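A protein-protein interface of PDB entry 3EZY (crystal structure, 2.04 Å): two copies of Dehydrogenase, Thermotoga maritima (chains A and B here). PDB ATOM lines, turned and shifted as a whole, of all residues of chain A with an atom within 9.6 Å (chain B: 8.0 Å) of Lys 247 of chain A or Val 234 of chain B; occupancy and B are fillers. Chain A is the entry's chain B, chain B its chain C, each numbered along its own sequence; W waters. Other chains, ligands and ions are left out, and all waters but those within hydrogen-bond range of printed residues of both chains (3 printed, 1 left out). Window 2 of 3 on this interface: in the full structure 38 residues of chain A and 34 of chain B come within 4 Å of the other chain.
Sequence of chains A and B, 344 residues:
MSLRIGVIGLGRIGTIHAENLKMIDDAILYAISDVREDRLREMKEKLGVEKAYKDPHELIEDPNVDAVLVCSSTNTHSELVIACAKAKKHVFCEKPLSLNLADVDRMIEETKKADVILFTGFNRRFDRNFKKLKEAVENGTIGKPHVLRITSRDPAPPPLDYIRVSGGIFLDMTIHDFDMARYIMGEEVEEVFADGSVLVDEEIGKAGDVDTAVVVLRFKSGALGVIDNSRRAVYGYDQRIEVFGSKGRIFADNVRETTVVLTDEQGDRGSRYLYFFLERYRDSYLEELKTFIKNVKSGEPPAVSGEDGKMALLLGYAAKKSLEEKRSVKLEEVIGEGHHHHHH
The guanidinium group (NH1) of Arg 232 of chain B lies within hydrogen-bond range of the backbone carbonyl oxygen (O) of Ser 246 of chain A, at 3.5 Å. The side-chain hydroxyl of Tyr 273 of chain B sits at hydrogen-bond distance from the guanidinium group of Arg 249 of chain A (3.0 Å).
The backbone carbonyl oxygen (O) of Ile 142 of chain A sits at hydrogen-bond distance from the backbone NH (N) of Ser 246 of chain A (3.2 Å). O of Lys 144 of chain A lies within hydrogen-bond range of N of Ser 246 of chain A. N of His 146 of chain A sits at hydrogen-bond distance from O of Phe 244 of chain A. N of Asp 154 of chain B sits at hydrogen-bond distance from O of Ser 230 of chain B (3.1 Å). O of Asp 154 of chain B sits at hydrogen-bond distance from N of Ala 233 of chain B, 2.8 Å away. N of Arg 232 of chain B lies within hydrogen-bond range of OG of Ser 230 of chain B (3.0 Å).
Phe 244 of chain A touches Arg 153 of chain B (CG to CZ, 3.6 Å). CE2 of Phe 244 of chain A touches OG of Ser 230 of chain B, 3.4 Å away. CZ of Phe 244 of chain A touches O of Arg 232 of chain B, 3.3 Å away. Ala 233 of chain B touches Phe 244 of chain A (CA to CE1, 3.9 Å). Phe 244 of chain A touches Tyr 235 of chain B (CD1 to OH, 3.8 Å). Ser 246 of chain A touches Val 234 of chain B. Lys 247 of chain A touches Val 234 of chain B (O to CG2, 3.6 Å). Gly 248 of chain A touches Val 234 of chain B (N to CG2, 3.9 Å). CD of Arg 249 of chain A touches NH1 of Arg 153 of chain B (3.95 Å). Arg 249 of chain A touches Tyr 235 of chain B (CD to OH, 3.6 Å).
Of chain B, only Val 234 comes within 4 Å of Lys 247 of chain A. Of chain A, only Ser 246 (3.4 Å), Lys 247 (3.6 Å) and Gly 248 (3.9 Å) come within 4 Å of Val 234 of chain B. Ala 233 of chain B touches one residue of chain A. Of the printed residues of chain A, Tyr 273 of chain B touches Arg 249. Printed residues of chain B within 4 Å of Gly 248 of chain A: Val 234 (3.9 Å). Of the printed residues of chain A, Arg 153 of chain B touches Phe 244 (3.6 Å) and Arg 249 (3.95 Å). Of the printed residues of chain B, Arg 249 of chain A touches Arg 153, Tyr 235 and Tyr 273. The nearest residue of chain A that does not touch Val 234 of chain B is Phe 244 of chain A (5.1 Å).
Of the 18 printed residues of chain A, 5 touch a printed residue of chain B. Printed residues of chain B that touch a printed residue of chain A: Arg 153, Ser 230, Arg 232, Ala 233, Val 234, Tyr 235 and Tyr 273.
No position is printed for both chains. Of the 12 pairs that touch across the chains among the printed residues, none has its exchanged pair printed and touching as well.
Water W1 bridges the backbone carbonyl oxygen of Arg 232 of chain B and a ring nitrogen (ND1) of His 146 of chain A. Water W2 lies within hydrogen-bond range of the side-chain hydroxyl of Ser 230 of chain B (2.7 Å) and a ring nitrogen (ND1) of His 146 of chain A (3.0 Å). Water W3 lies within hydrogen-bond range of OH of Tyr 273 of chain B (2.8 Å) and NH1 of Arg 249 of chain A (3.0 Å).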
ATOM      1  N   ALA A 136       8.139 -16.380 -10.502  1.00  0.00           N
ATOM      2  CA  ALA A 136       9.346 -16.523 -11.323  1.00  0.00           C
ATOM      3  C   ALA A 136       9.106 -17.100 -12.737  1.00  0.00           C
ATOM      4  O   ALA A 136       9.652 -16.610 -13.734  1.00  0.00           O
ATOM      5  CB  ALA A 136      10.378 -17.363 -10.606  1.00  0.00           C
ATOM      6  N   VAL A 137       8.312 -18.157 -12.825  1.00  0.00           N
ATOM      7  CA  VAL A 137       7.998 -18.749 -14.131  1.00  0.00           C
ATOM      8  C   VAL A 137       7.278 -17.697 -15.023  1.00  0.00           C
ATOM      9  O   VAL A 137       7.618 -17.500 -16.201  1.00  0.00           O
ATOM     10  CB  VAL A 137       7.193 -20.044 -13.960  1.00  0.00           C
ATOM     11  CG1 VAL A 137       6.637 -20.549 -15.308  1.00  0.00           C
ATOM     12  CG2 VAL A 137       8.077 -21.162 -13.269  1.00  0.00           C
ATOM     13  N   ASN A 139       7.411 -14.411 -14.779  1.00  0.00           N
ATOM     14  CA  ASN A 139       8.339 -13.360 -15.176  1.00  0.00           C
ATOM     15  C   ASN A 139       9.294 -13.772 -16.286  1.00  0.00           C
ATOM     16  O   ASN A 139      10.097 -12.947 -16.706  1.00  0.00           O
ATOM     17  CB  ASN A 139       9.182 -12.898 -13.983  1.00  0.00           C
ATOM     18  CG  ASN A 139       8.372 -12.178 -12.958  1.00  0.00           C
ATOM     19  OD1 ASN A 139       7.233 -11.787 -13.214  1.00  0.00           O
ATOM     20  ND2 ASN A 139       8.930 -12.014 -11.774  1.00  0.00           N
ATOM     21  N   GLY A 140       9.254 -15.032 -16.727  1.00  0.00           N
ATOM     22  CA  GLY A 140      10.159 -15.506 -17.806  1.00  0.00           C
ATOM     23  C   GLY A 140      11.542 -16.028 -17.397  1.00  0.00           C
ATOM     24  O   GLY A 140      12.387 -16.268 -18.253  1.00  0.00           O
ATOM     25  N   THR A 141      11.777 -16.234 -16.095  1.00  0.00           N
ATOM     26  CA  THR A 141      13.116 -16.629 -15.629  1.00  0.00           C
ATOM     27  C   THR A 141      13.586 -18.009 -16.120  1.00  0.00           C
ATOM     28  O   THR A 141      14.776 -18.279 -16.121  1.00  0.00           O
ATOM     29  CB  THR A 141      13.220 -16.615 -14.070  1.00  0.00           C
ATOM     30  OG1 THR A 141      12.544 -17.779 -13.530  1.00  0.00           O
ATOM     31  CG2 THR A 141      12.615 -15.319 -13.518  1.00  0.00           C
ATOM     32  N   ILE A 142      12.691 -18.903 -16.522  1.00  0.00           N
ATOM     33  CA  ILE A 142      13.170 -20.152 -17.123  1.00  0.00           C
ATOM     34  C   ILE A 142      12.829 -20.243 -18.632  1.00  0.00           C
ATOM     35  O   ILE A 142      12.825 -21.319 -19.211  1.00  0.00           O
ATOM     36  CB  ILE A 142      12.675 -21.400 -16.363  1.00  0.00           C
ATOM     37  CG1 ILE A 142      11.151 -21.392 -16.225  1.00  0.00           C
ATOM     38  CG2 ILE A 142      13.314 -21.460 -14.947  1.00  0.00           C
ATOM     39  CD1 ILE A 142      10.399 -22.125 -17.312  1.00  0.00           C
ATOM     40  N   GLY A 143      12.588 -19.090 -19.249  1.00  0.00           N
ATOM     41  CA  GLY A 143      12.052 -19.009 -20.607  1.00  0.00           C
ATOM     42  C   GLY A 143      10.728 -19.737 -20.796  1.00  0.00           C
ATOM     43  O   GLY A 143       9.845 -19.690 -19.959  1.00  0.00           O
ATOM     44  N   LYS A 144      10.576 -20.394 -21.915  1.00  0.00           N
ATOM     45  CA  LYS A 144       9.363 -21.095 -22.233  1.00  0.00           C
ATOM     46  C   LYS A 144       9.372 -22.430 -21.487  1.00  0.00           C
ATOM     47  O   LYS A 144      10.297 -23.192 -21.640  1.00  0.00           O
ATOM     48  CB  LYS A 144       9.309 -21.369 -23.741  1.00  0.00           C
ATOM     49  CG  LYS A 144       8.017 -22.091 -24.180  1.00  0.00           C
ATOM     50  CD  LYS A 144       7.954 -22.216 -25.706  1.00  0.00           C
ATOM     51  CE  LYS A 144       6.601 -22.761 -26.177  1.00  0.00           C
ATOM     52  NZ  LYS A 144       6.648 -22.961 -27.651  1.00  0.00           N
ATOM     53  N   PRO A 145       8.329 -22.694 -20.681  1.00  0.00           N
ATOM     54  CA  PRO A 145       8.173 -23.947 -19.914  1.00  0.00           C
ATOM     55  C   PRO A 145       8.073 -25.125 -20.878  1.00  0.00           C
ATOM     56  O   PRO A 145       7.350 -25.017 -21.875  1.00  0.00           O
ATOM     57  CB  PRO A 145       6.830 -23.752 -19.207  1.00  0.00           C
ATOM     58  CG  PRO A 145       6.609 -22.219 -19.166  1.00  0.00           C
ATOM     59  CD  PRO A 145       7.250 -21.719 -20.419  1.00  0.00           C
ATOM     60  N   HIS A 146       8.761 -26.231 -20.573  1.00  0.00           N
ATOM     61  CA  HIS A 146       8.747 -27.407 -21.395  1.00  0.00           C
ATOM     62  C   HIS A 146       8.171 -28.594 -20.644  1.00  0.00           C
ATOM     63  O   HIS A 146       7.431 -29.408 -21.236  1.00  0.00           O
ATOM     64  CB  HIS A 146      10.178 -27.761 -21.867  1.00  0.00           C
ATOM     65  CG  HIS A 146      10.666 -26.873 -22.967  1.00  0.00           C
ATOM     66  ND1 HIS A 146      11.831 -27.102 -23.659  1.00  0.00           N
ATOM     67  CD2 HIS A 146      10.112 -25.765 -23.519  1.00  0.00           C
ATOM     68  CE1 HIS A 146      12.000 -26.150 -24.556  1.00  0.00           C
ATOM     69  NE2 HIS A 146      10.969 -25.328 -24.496  1.00  0.00           N
ATOM     70  N   VAL A 243       9.843 -26.789 -12.574  1.00  0.00           N
ATOM     71  CA  VAL A 243       9.502 -26.421 -13.969  1.00  0.00           C
ATOM     72  C   VAL A 243      10.790 -26.315 -14.783  1.00  0.00           C
ATOM     73  O   VAL A 243      11.751 -25.631 -14.366  1.00  0.00           O
ATOM     74  CB  VAL A 243       8.718 -25.073 -14.042  1.00  0.00           C
ATOM     75  CG1 VAL A 243       8.455 -24.682 -15.531  1.00  0.00           C
ATOM     76  CG2 VAL A 243       7.382 -25.166 -13.235  1.00  0.00           C
ATOM     77  N   PHE A 244      10.844 -26.994 -15.924  1.00  0.00           N
ATOM     78  CA  PHE A 244      12.041 -26.947 -16.764  1.00  0.00           C
ATOM     79  C   PHE A 244      11.666 -26.254 -18.060  1.00  0.00           C
ATOM     80  O   PHE A 244      10.621 -26.561 -18.639  1.00  0.00           O
ATOM     81  CB  PHE A 244      12.502 -28.372 -17.068  1.00  0.00           C
ATOM     82  CG  PHE A 244      13.475 -28.483 -18.241  1.00  0.00           C
ATOM     83  CD1 PHE A 244      14.779 -28.035 -18.128  1.00  0.00           C
ATOM     84  CD2 PHE A 244      13.070 -29.055 -19.442  1.00  0.00           C
ATOM     85  CE1 PHE A 244      15.662 -28.135 -19.208  1.00  0.00           C
ATOM     86  CE2 PHE A 244      13.956 -29.177 -20.527  1.00  0.00           C
ATOM     87  CZ  PHE A 244      15.235 -28.724 -20.407  1.00  0.00           C
ATOM     88  N   GLY A 245      12.493 -25.340 -18.545  1.00  0.00           N
ATOM     89  CA  GLY A 245      12.161 -24.711 -19.817  1.00  0.00           C
ATOM     90  C   GLY A 245      13.376 -24.276 -20.606  1.00  0.00           C
ATOM     91  O   GLY A 245      14.494 -24.671 -20.296  1.00  0.00           O
ATOM     92  N   SER A 246      13.176 -23.428 -21.615  1.00  0.00           N
ATOM     93  CA  SER A 246      14.246 -23.182 -22.551  1.00  0.00           C
ATOM     94  C   SER A 246      15.471 -22.474 -21.956  1.00  0.00           C
ATOM     95  O   SER A 246      16.553 -22.548 -22.536  1.00  0.00           O
ATOM     96  CB  SER A 246      13.720 -22.425 -23.785  1.00  0.00           C
ATOM     97  OG  SER A 246      13.220 -21.131 -23.430  1.00  0.00           O
ATOM     98  N   LYS A 247      15.304 -21.768 -20.837  1.00  0.00           N
ATOM     99  CA  LYS A 247      16.392 -20.980 -20.243  1.00  0.00           C
ATOM    100  C   LYS A 247      16.860 -21.528 -18.885  1.00  0.00           C
ATOM    101  O   LYS A 247      17.755 -20.959 -18.250  1.00  0.00           O
ATOM    102  CB  LYS A 247      15.984 -19.498 -20.054  1.00  0.00           C
ATOM    103  CG  LYS A 247      15.931 -18.726 -21.356  1.00  0.00           C
ATOM    104  CD  LYS A 247      15.307 -17.363 -21.124  1.00  0.00           C
ATOM    105  CE  LYS A 247      14.495 -16.909 -22.387  1.00  0.00           C
ATOM    106  NZ  LYS A 247      13.941 -15.514 -22.333  1.00  0.00           N
ATOM    107  N   GLY A 248      16.280 -22.619 -18.424  1.00  0.00           N
ATOM    108  CA  GLY A 248      16.783 -23.187 -17.159  1.00  0.00           C
ATOM    109  C   GLY A 248      15.765 -24.016 -16.420  1.00  0.00           C
ATOM    110  O   GLY A 248      14.772 -24.455 -17.002  1.00  0.00           O
ATOM    111  N   ARG A 249      15.999 -24.230 -15.137  1.00  0.00           N
ATOM    112  CA  ARG A 249      15.105 -25.069 -14.326  1.00  0.00           C
ATOM    113  C   ARG A 249      14.816 -24.320 -13.066  1.00  0.00           C
ATOM    114  O   ARG A 249      15.686 -23.593 -12.552  1.00  0.00           O
ATOM    115  CB  ARG A 249      15.814 -26.381 -13.978  1.00  0.00           C
ATOM    116  CG  ARG A 249      14.968 -27.387 -13.211  1.00  0.00           C
ATOM    117  CD  ARG A 249      15.871 -28.541 -12.721  1.00  0.00           C
ATOM    118  NE  ARG A 249      16.591 -28.163 -11.515  1.00  0.00           N
ATOM    119  CZ  ARG A 249      17.646 -28.819 -11.041  1.00  0.00           C
ATOM    120  NH1 ARG A 249      18.162 -29.864 -11.704  1.00  0.00           N
ATOM    121  NH2 ARG A 249      18.189 -28.413  -9.912  1.00  0.00           N
ATOM    122  N   ILE A 250      13.609 -24.468 -12.540  1.00  0.00           N
ATOM    123  CA  ILE A 250      13.281 -23.895 -11.221  1.00  0.00           C
ATOM    124  C   ILE A 250      12.563 -24.939 -10.315  1.00  0.00           C
ATOM    125  O   ILE A 250      11.805 -25.761 -10.812  1.00  0.00           O
ATOM    126  CB  ILE A 250      12.502 -22.593 -11.400  1.00  0.00           C
ATOM    127  CG1 ILE A 250      12.455 -21.799 -10.082  1.00  0.00           C
ATOM    128  CG2 ILE A 250      11.111 -22.845 -12.070  1.00  0.00           C
ATOM    129  CD1 ILE A 250      11.889 -20.402 -10.218  1.00  0.00           C
ATOM    130  N   ARG B 153      18.426 -35.277 -19.214  1.00  0.00           N
ATOM    131  CA  ARG B 153      18.451 -34.173 -20.175  1.00  0.00           C
ATOM    132  C   ARG B 153      19.912 -33.988 -20.621  1.00  0.00           C
ATOM    133  O   ARG B 153      20.832 -34.032 -19.779  1.00  0.00           O
ATOM    134  CB  ARG B 153      17.925 -32.894 -19.528  1.00  0.00           C
ATOM    135  CG  ARG B 153      16.486 -33.018 -18.992  1.00  0.00           C
ATOM    136  CD  ARG B 153      15.967 -31.762 -18.293  1.00  0.00           C
ATOM    137  NE  ARG B 153      14.605 -32.004 -17.796  1.00  0.00           N
ATOM    138  CZ  ARG B 153      14.137 -31.582 -16.612  1.00  0.00           C
ATOM    139  NH1 ARG B 153      14.874 -30.801 -15.808  1.00  0.00           N
ATOM    140  NH2 ARG B 153      12.895 -31.890 -16.252  1.00  0.00           N
ATOM    141  N   ASP B 154      20.131 -33.850 -21.924  1.00  0.00           N
ATOM    142  CA  ASP B 154      21.454 -33.516 -22.460  1.00  0.00           C
ATOM    143  C   ASP B 154      21.549 -32.026 -22.731  1.00  0.00           C
ATOM    144  O   ASP B 154      20.518 -31.347 -22.912  1.00  0.00           O
ATOM    145  CB  ASP B 154      21.745 -34.267 -23.777  1.00  0.00           C
ATOM    146  CG  ASP B 154      21.861 -35.776 -23.600  1.00  0.00           C
ATOM    147  OD1 ASP B 154      22.098 -36.269 -22.475  1.00  0.00           O
ATOM    148  OD2 ASP B 154      21.696 -36.491 -24.617  1.00  0.00           O
ATOM    149  N   PRO B 155      22.789 -31.501 -22.805  1.00  0.00           N
ATOM    150  CA  PRO B 155      22.934 -30.067 -23.045  1.00  0.00           C
ATOM    151  C   PRO B 155      22.596 -29.639 -24.471  1.00  0.00           C
ATOM    152  O   PRO B 155      22.262 -28.501 -24.684  1.00  0.00           O
ATOM    153  CB  PRO B 155      24.410 -29.780 -22.770  1.00  0.00           C
ATOM    154  CG  PRO B 155      25.020 -31.041 -22.303  1.00  0.00           C
ATOM    155  CD  PRO B 155      24.013 -32.112 -22.240  1.00  0.00           C
ATOM    156  N   ALA B 156      22.707 -30.543 -25.435  1.00  0.00           N
ATOM    157  CA  ALA B 156      22.384 -30.214 -26.829  1.00  0.00           C
ATOM    158  C   ALA B 156      21.955 -31.470 -27.607  1.00  0.00           C
ATOM    159  O   ALA B 156      22.313 -32.611 -27.240  1.00  0.00           O
ATOM    160  CB  ALA B 156      23.573 -29.533 -27.526  1.00  0.00           C
ATOM    161  N   SER B 230      14.893 -34.550 -22.284  1.00  0.00           N
ATOM    162  CA  SER B 230      14.933 -33.371 -23.150  1.00  0.00           C
ATOM    163  C   SER B 230      16.242 -33.423 -23.871  1.00  0.00           C
ATOM    164  O   SER B 230      17.290 -33.688 -23.252  1.00  0.00           O
ATOM    165  CB  SER B 230      14.957 -32.088 -22.332  1.00  0.00           C
ATOM    166  OG  SER B 230      15.149 -30.948 -23.166  1.00  0.00           O
ATOM    167  N   ARG B 231      16.211 -33.081 -25.150  1.00  0.00           N
ATOM    168  CA  ARG B 231      17.437 -32.957 -25.934  1.00  0.00           C
ATOM    169  C   ARG B 231      18.234 -31.688 -25.628  1.00  0.00           C
ATOM    170  O   ARG B 231      19.307 -31.503 -26.180  1.00  0.00           O
ATOM    171  CB  ARG B 231      17.082 -32.982 -27.434  1.00  0.00           C
ATOM    172  CG  ARG B 231      16.615 -34.348 -27.931  1.00  0.00           C
ATOM    173  CD  ARG B 231      17.813 -35.219 -28.178  1.00  0.00           C
ATOM    174  NE  ARG B 231      17.508 -36.498 -28.830  1.00  0.00           N
ATOM    175  CZ  ARG B 231      18.328 -37.535 -28.733  1.00  0.00           C
ATOM    176  NH1 ARG B 231      19.442 -37.390 -28.025  1.00  0.00           N
ATOM    177  NH2 ARG B 231      18.063 -38.689 -29.321  1.00  0.00           N
ATOM    178  N   ARG B 232      17.724 -30.792 -24.786  1.00  0.00           N
ATOM    179  CA  ARG B 232      18.452 -29.531 -24.542  1.00  0.00           C
ATOM    180  C   ARG B 232      18.237 -28.861 -23.178  1.00  0.00           C
ATOM    181  O   ARG B 232      17.207 -28.236 -22.947  1.00  0.00           O
ATOM    182  CB  ARG B 232      18.185 -28.479 -25.640  1.00  0.00           C
ATOM    183  CG  ARG B 232      19.004 -27.187 -25.407  1.00  0.00           C
ATOM    184  CD  ARG B 232      18.836 -26.230 -26.543  1.00  0.00           C
ATOM    185  NE  ARG B 232      19.631 -25.012 -26.389  1.00  0.00           N
ATOM    186  CZ  ARG B 232      19.159 -23.863 -25.906  1.00  0.00           C
ATOM    187  NH1 ARG B 232      17.897 -23.774 -25.488  1.00  0.00           N
ATOM    188  NH2 ARG B 232      19.951 -22.798 -25.817  1.00  0.00           N
ATOM    189  N   ALA B 233      19.233 -28.943 -22.305  1.00  0.00           N
ATOM    190  CA  ALA B 233      19.156 -28.328 -20.992  1.00  0.00           C
ATOM    191  C   ALA B 233      20.301 -27.377 -20.995  1.00  0.00           C
ATOM    192  O   ALA B 233      21.458 -27.817 -20.961  1.00  0.00           O
ATOM    193  CB  ALA B 233      19.359 -29.380 -19.878  1.00  0.00           C
ATOM    194  N   VAL B 234      20.016 -26.082 -21.015  1.00  0.00           N
ATOM    195  CA  VAL B 234      21.106 -25.106 -21.169  1.00  0.00           C
ATOM    196  C   VAL B 234      22.101 -25.123 -19.999  1.00  0.00           C
ATOM    197  O   VAL B 234      23.228 -24.678 -20.144  1.00  0.00           O
ATOM    198  CB  VAL B 234      20.593 -23.663 -21.366  1.00  0.00           C
ATOM    199  CG1 VAL B 234      19.804 -23.568 -22.657  1.00  0.00           C
ATOM    200  CG2 VAL B 234      19.744 -23.241 -20.169  1.00  0.00           C
ATOM    201  N   TYR B 235      21.691 -25.644 -18.846  1.00  0.00           N
ATOM    202  CA  TYR B 235      22.588 -25.648 -17.700  1.00  0.00           C
ATOM    203  C   TYR B 235      23.588 -26.811 -17.624  1.00  0.00           C
ATOM    204  O   TYR B 235      24.448 -26.847 -16.714  1.00  0.00           O
ATOM    205  CB  TYR B 235      21.775 -25.496 -16.386  1.00  0.00           C
ATOM    206  CG  TYR B 235      20.651 -26.514 -16.229  1.00  0.00           C
ATOM    207  CD1 TYR B 235      20.854 -27.707 -15.545  1.00  0.00           C
ATOM    208  CD2 TYR B 235      19.382 -26.271 -16.768  1.00  0.00           C
ATOM    209  CE1 TYR B 235      19.814 -28.614 -15.378  1.00  0.00           C
ATOM    210  CE2 TYR B 235      18.354 -27.188 -16.653  1.00  0.00           C
ATOM    211  CZ  TYR B 235      18.572 -28.360 -15.962  1.00  0.00           C
ATOM    212  OH  TYR B 235      17.530 -29.269 -15.811  1.00  0.00           O
ATOM    213  N   GLY B 236      23.522 -27.751 -18.569  1.00  0.00           N
ATOM    214  CA  GLY B 236      24.388 -28.933 -18.522  1.00  0.00           C
ATOM    215  C   GLY B 236      23.594 -30.224 -18.468  1.00  0.00           C
ATOM    216  O   GLY B 236      22.366 -30.213 -18.666  1.00  0.00           O
ATOM    217  N   TYR B 237      24.272 -31.347 -18.239  1.00  0.00           N
ATOM    218  CA  TYR B 237      23.573 -32.623 -18.120  1.00  0.00           C
ATOM    219  C   TYR B 237      22.644 -32.539 -16.928  1.00  0.00           C
ATOM    220  O   TYR B 237      23.011 -32.011 -15.874  1.00  0.00           O
ATOM    221  CB  TYR B 237      24.554 -33.791 -17.918  1.00  0.00           C
ATOM    222  CG  TYR B 237      25.290 -34.187 -19.165  1.00  0.00           C
ATOM    223  CD1 TYR B 237      24.680 -34.979 -20.123  1.00  0.00           C
ATOM    224  CD2 TYR B 237      26.603 -33.754 -19.401  1.00  0.00           C
ATOM    225  CE1 TYR B 237      25.342 -35.338 -21.282  1.00  0.00           C
ATOM    226  CE2 TYR B 237      27.273 -34.123 -20.559  1.00  0.00           C
ATOM    227  CZ  TYR B 237      26.634 -34.912 -21.479  1.00  0.00           C
ATOM    228  OH  TYR B 237      27.276 -35.271 -22.641  1.00  0.00           O
ATOM    229  N   TYR B 273      27.051 -27.068 -13.410  1.00  0.00           N
ATOM    230  CA  TYR B 273      26.890 -28.516 -13.568  1.00  0.00           C
ATOM    231  C   TYR B 273      27.938 -29.031 -14.552  1.00  0.00           C
ATOM    232  O   TYR B 273      28.451 -28.272 -15.383  1.00  0.00           O
ATOM    233  CB  TYR B 273      25.487 -28.851 -14.152  1.00  0.00           C
ATOM    234  CG  TYR B 273      24.305 -28.695 -13.168  1.00  0.00           C
ATOM    235  CD1 TYR B 273      24.294 -27.678 -12.212  1.00  0.00           C
ATOM    236  CD2 TYR B 273      23.225 -29.566 -13.199  1.00  0.00           C
ATOM    237  CE1 TYR B 273      23.222 -27.529 -11.307  1.00  0.00           C
ATOM    238  CE2 TYR B 273      22.148 -29.431 -12.297  1.00  0.00           C
ATOM    239  CZ  TYR B 273      22.141 -28.409 -11.374  1.00  0.00           C
ATOM    240  OH  TYR B 273      21.081 -28.283 -10.485  1.00  0.00           O
ATOM    241  N   LEU B 274      28.222 -30.323 -14.506  1.00  0.00           N
ATOM    242  CA  LEU B 274      29.041 -30.901 -15.563  1.00  0.00           C
ATOM    243  C   LEU B 274      28.308 -30.708 -16.889  1.00  0.00           C
ATOM    244  O   LEU B 274      27.078 -30.829 -16.961  1.00  0.00           O
ATOM    245  CB  LEU B 274      29.297 -32.376 -15.291  1.00  0.00           C
ATOM    246  CG  LEU B 274      30.072 -32.619 -14.004  1.00  0.00           C
ATOM    247  CD1 LEU B 274      30.556 -34.089 -14.023  1.00  0.00           C
ATOM    248  CD2 LEU B 274      31.253 -31.613 -13.781  1.00  0.00           C
ATOM    249  N   TYR B 275      29.066 -30.369 -17.916  1.00  0.00           N
ATOM    250  CA  TYR B 275      28.524 -29.894 -19.182  1.00  0.00           C
ATOM    251  C   TYR B 275      29.102 -30.668 -20.383  1.00  0.00           C
ATOM    252  O   TYR B 275      28.383 -30.943 -21.361  1.00  0.00           O
ATOM    253  CB  TYR B 275      28.832 -28.391 -19.340  1.00  0.00           C
ATOM    254  CG  TYR B 275      28.108 -27.759 -20.493  1.00  0.00           C
ATOM    255  CD1 TYR B 275      26.895 -27.088 -20.300  1.00  0.00           C
ATOM    256  CD2 TYR B 275      28.617 -27.847 -21.785  1.00  0.00           C
ATOM    257  CE1 TYR B 275      26.208 -26.508 -21.361  1.00  0.00           C
ATOM    258  CE2 TYR B 275      27.931 -27.266 -22.867  1.00  0.00           C
ATOM    259  CZ  TYR B 275      26.728 -26.608 -22.639  1.00  0.00           C
ATOM    260  OH  TYR B 275      26.056 -26.036 -23.698  1.00  0.00           O
HETATM  261  O   HOH W   1      15.191 -26.732 -23.756  1.00  0.00           O
HETATM  262  O   HOH W   2      12.699 -29.931 -23.812  1.00  0.00           O
HETATM  263  O   HOH W   3      20.371 -30.936  -9.948  1.00  0.00           O
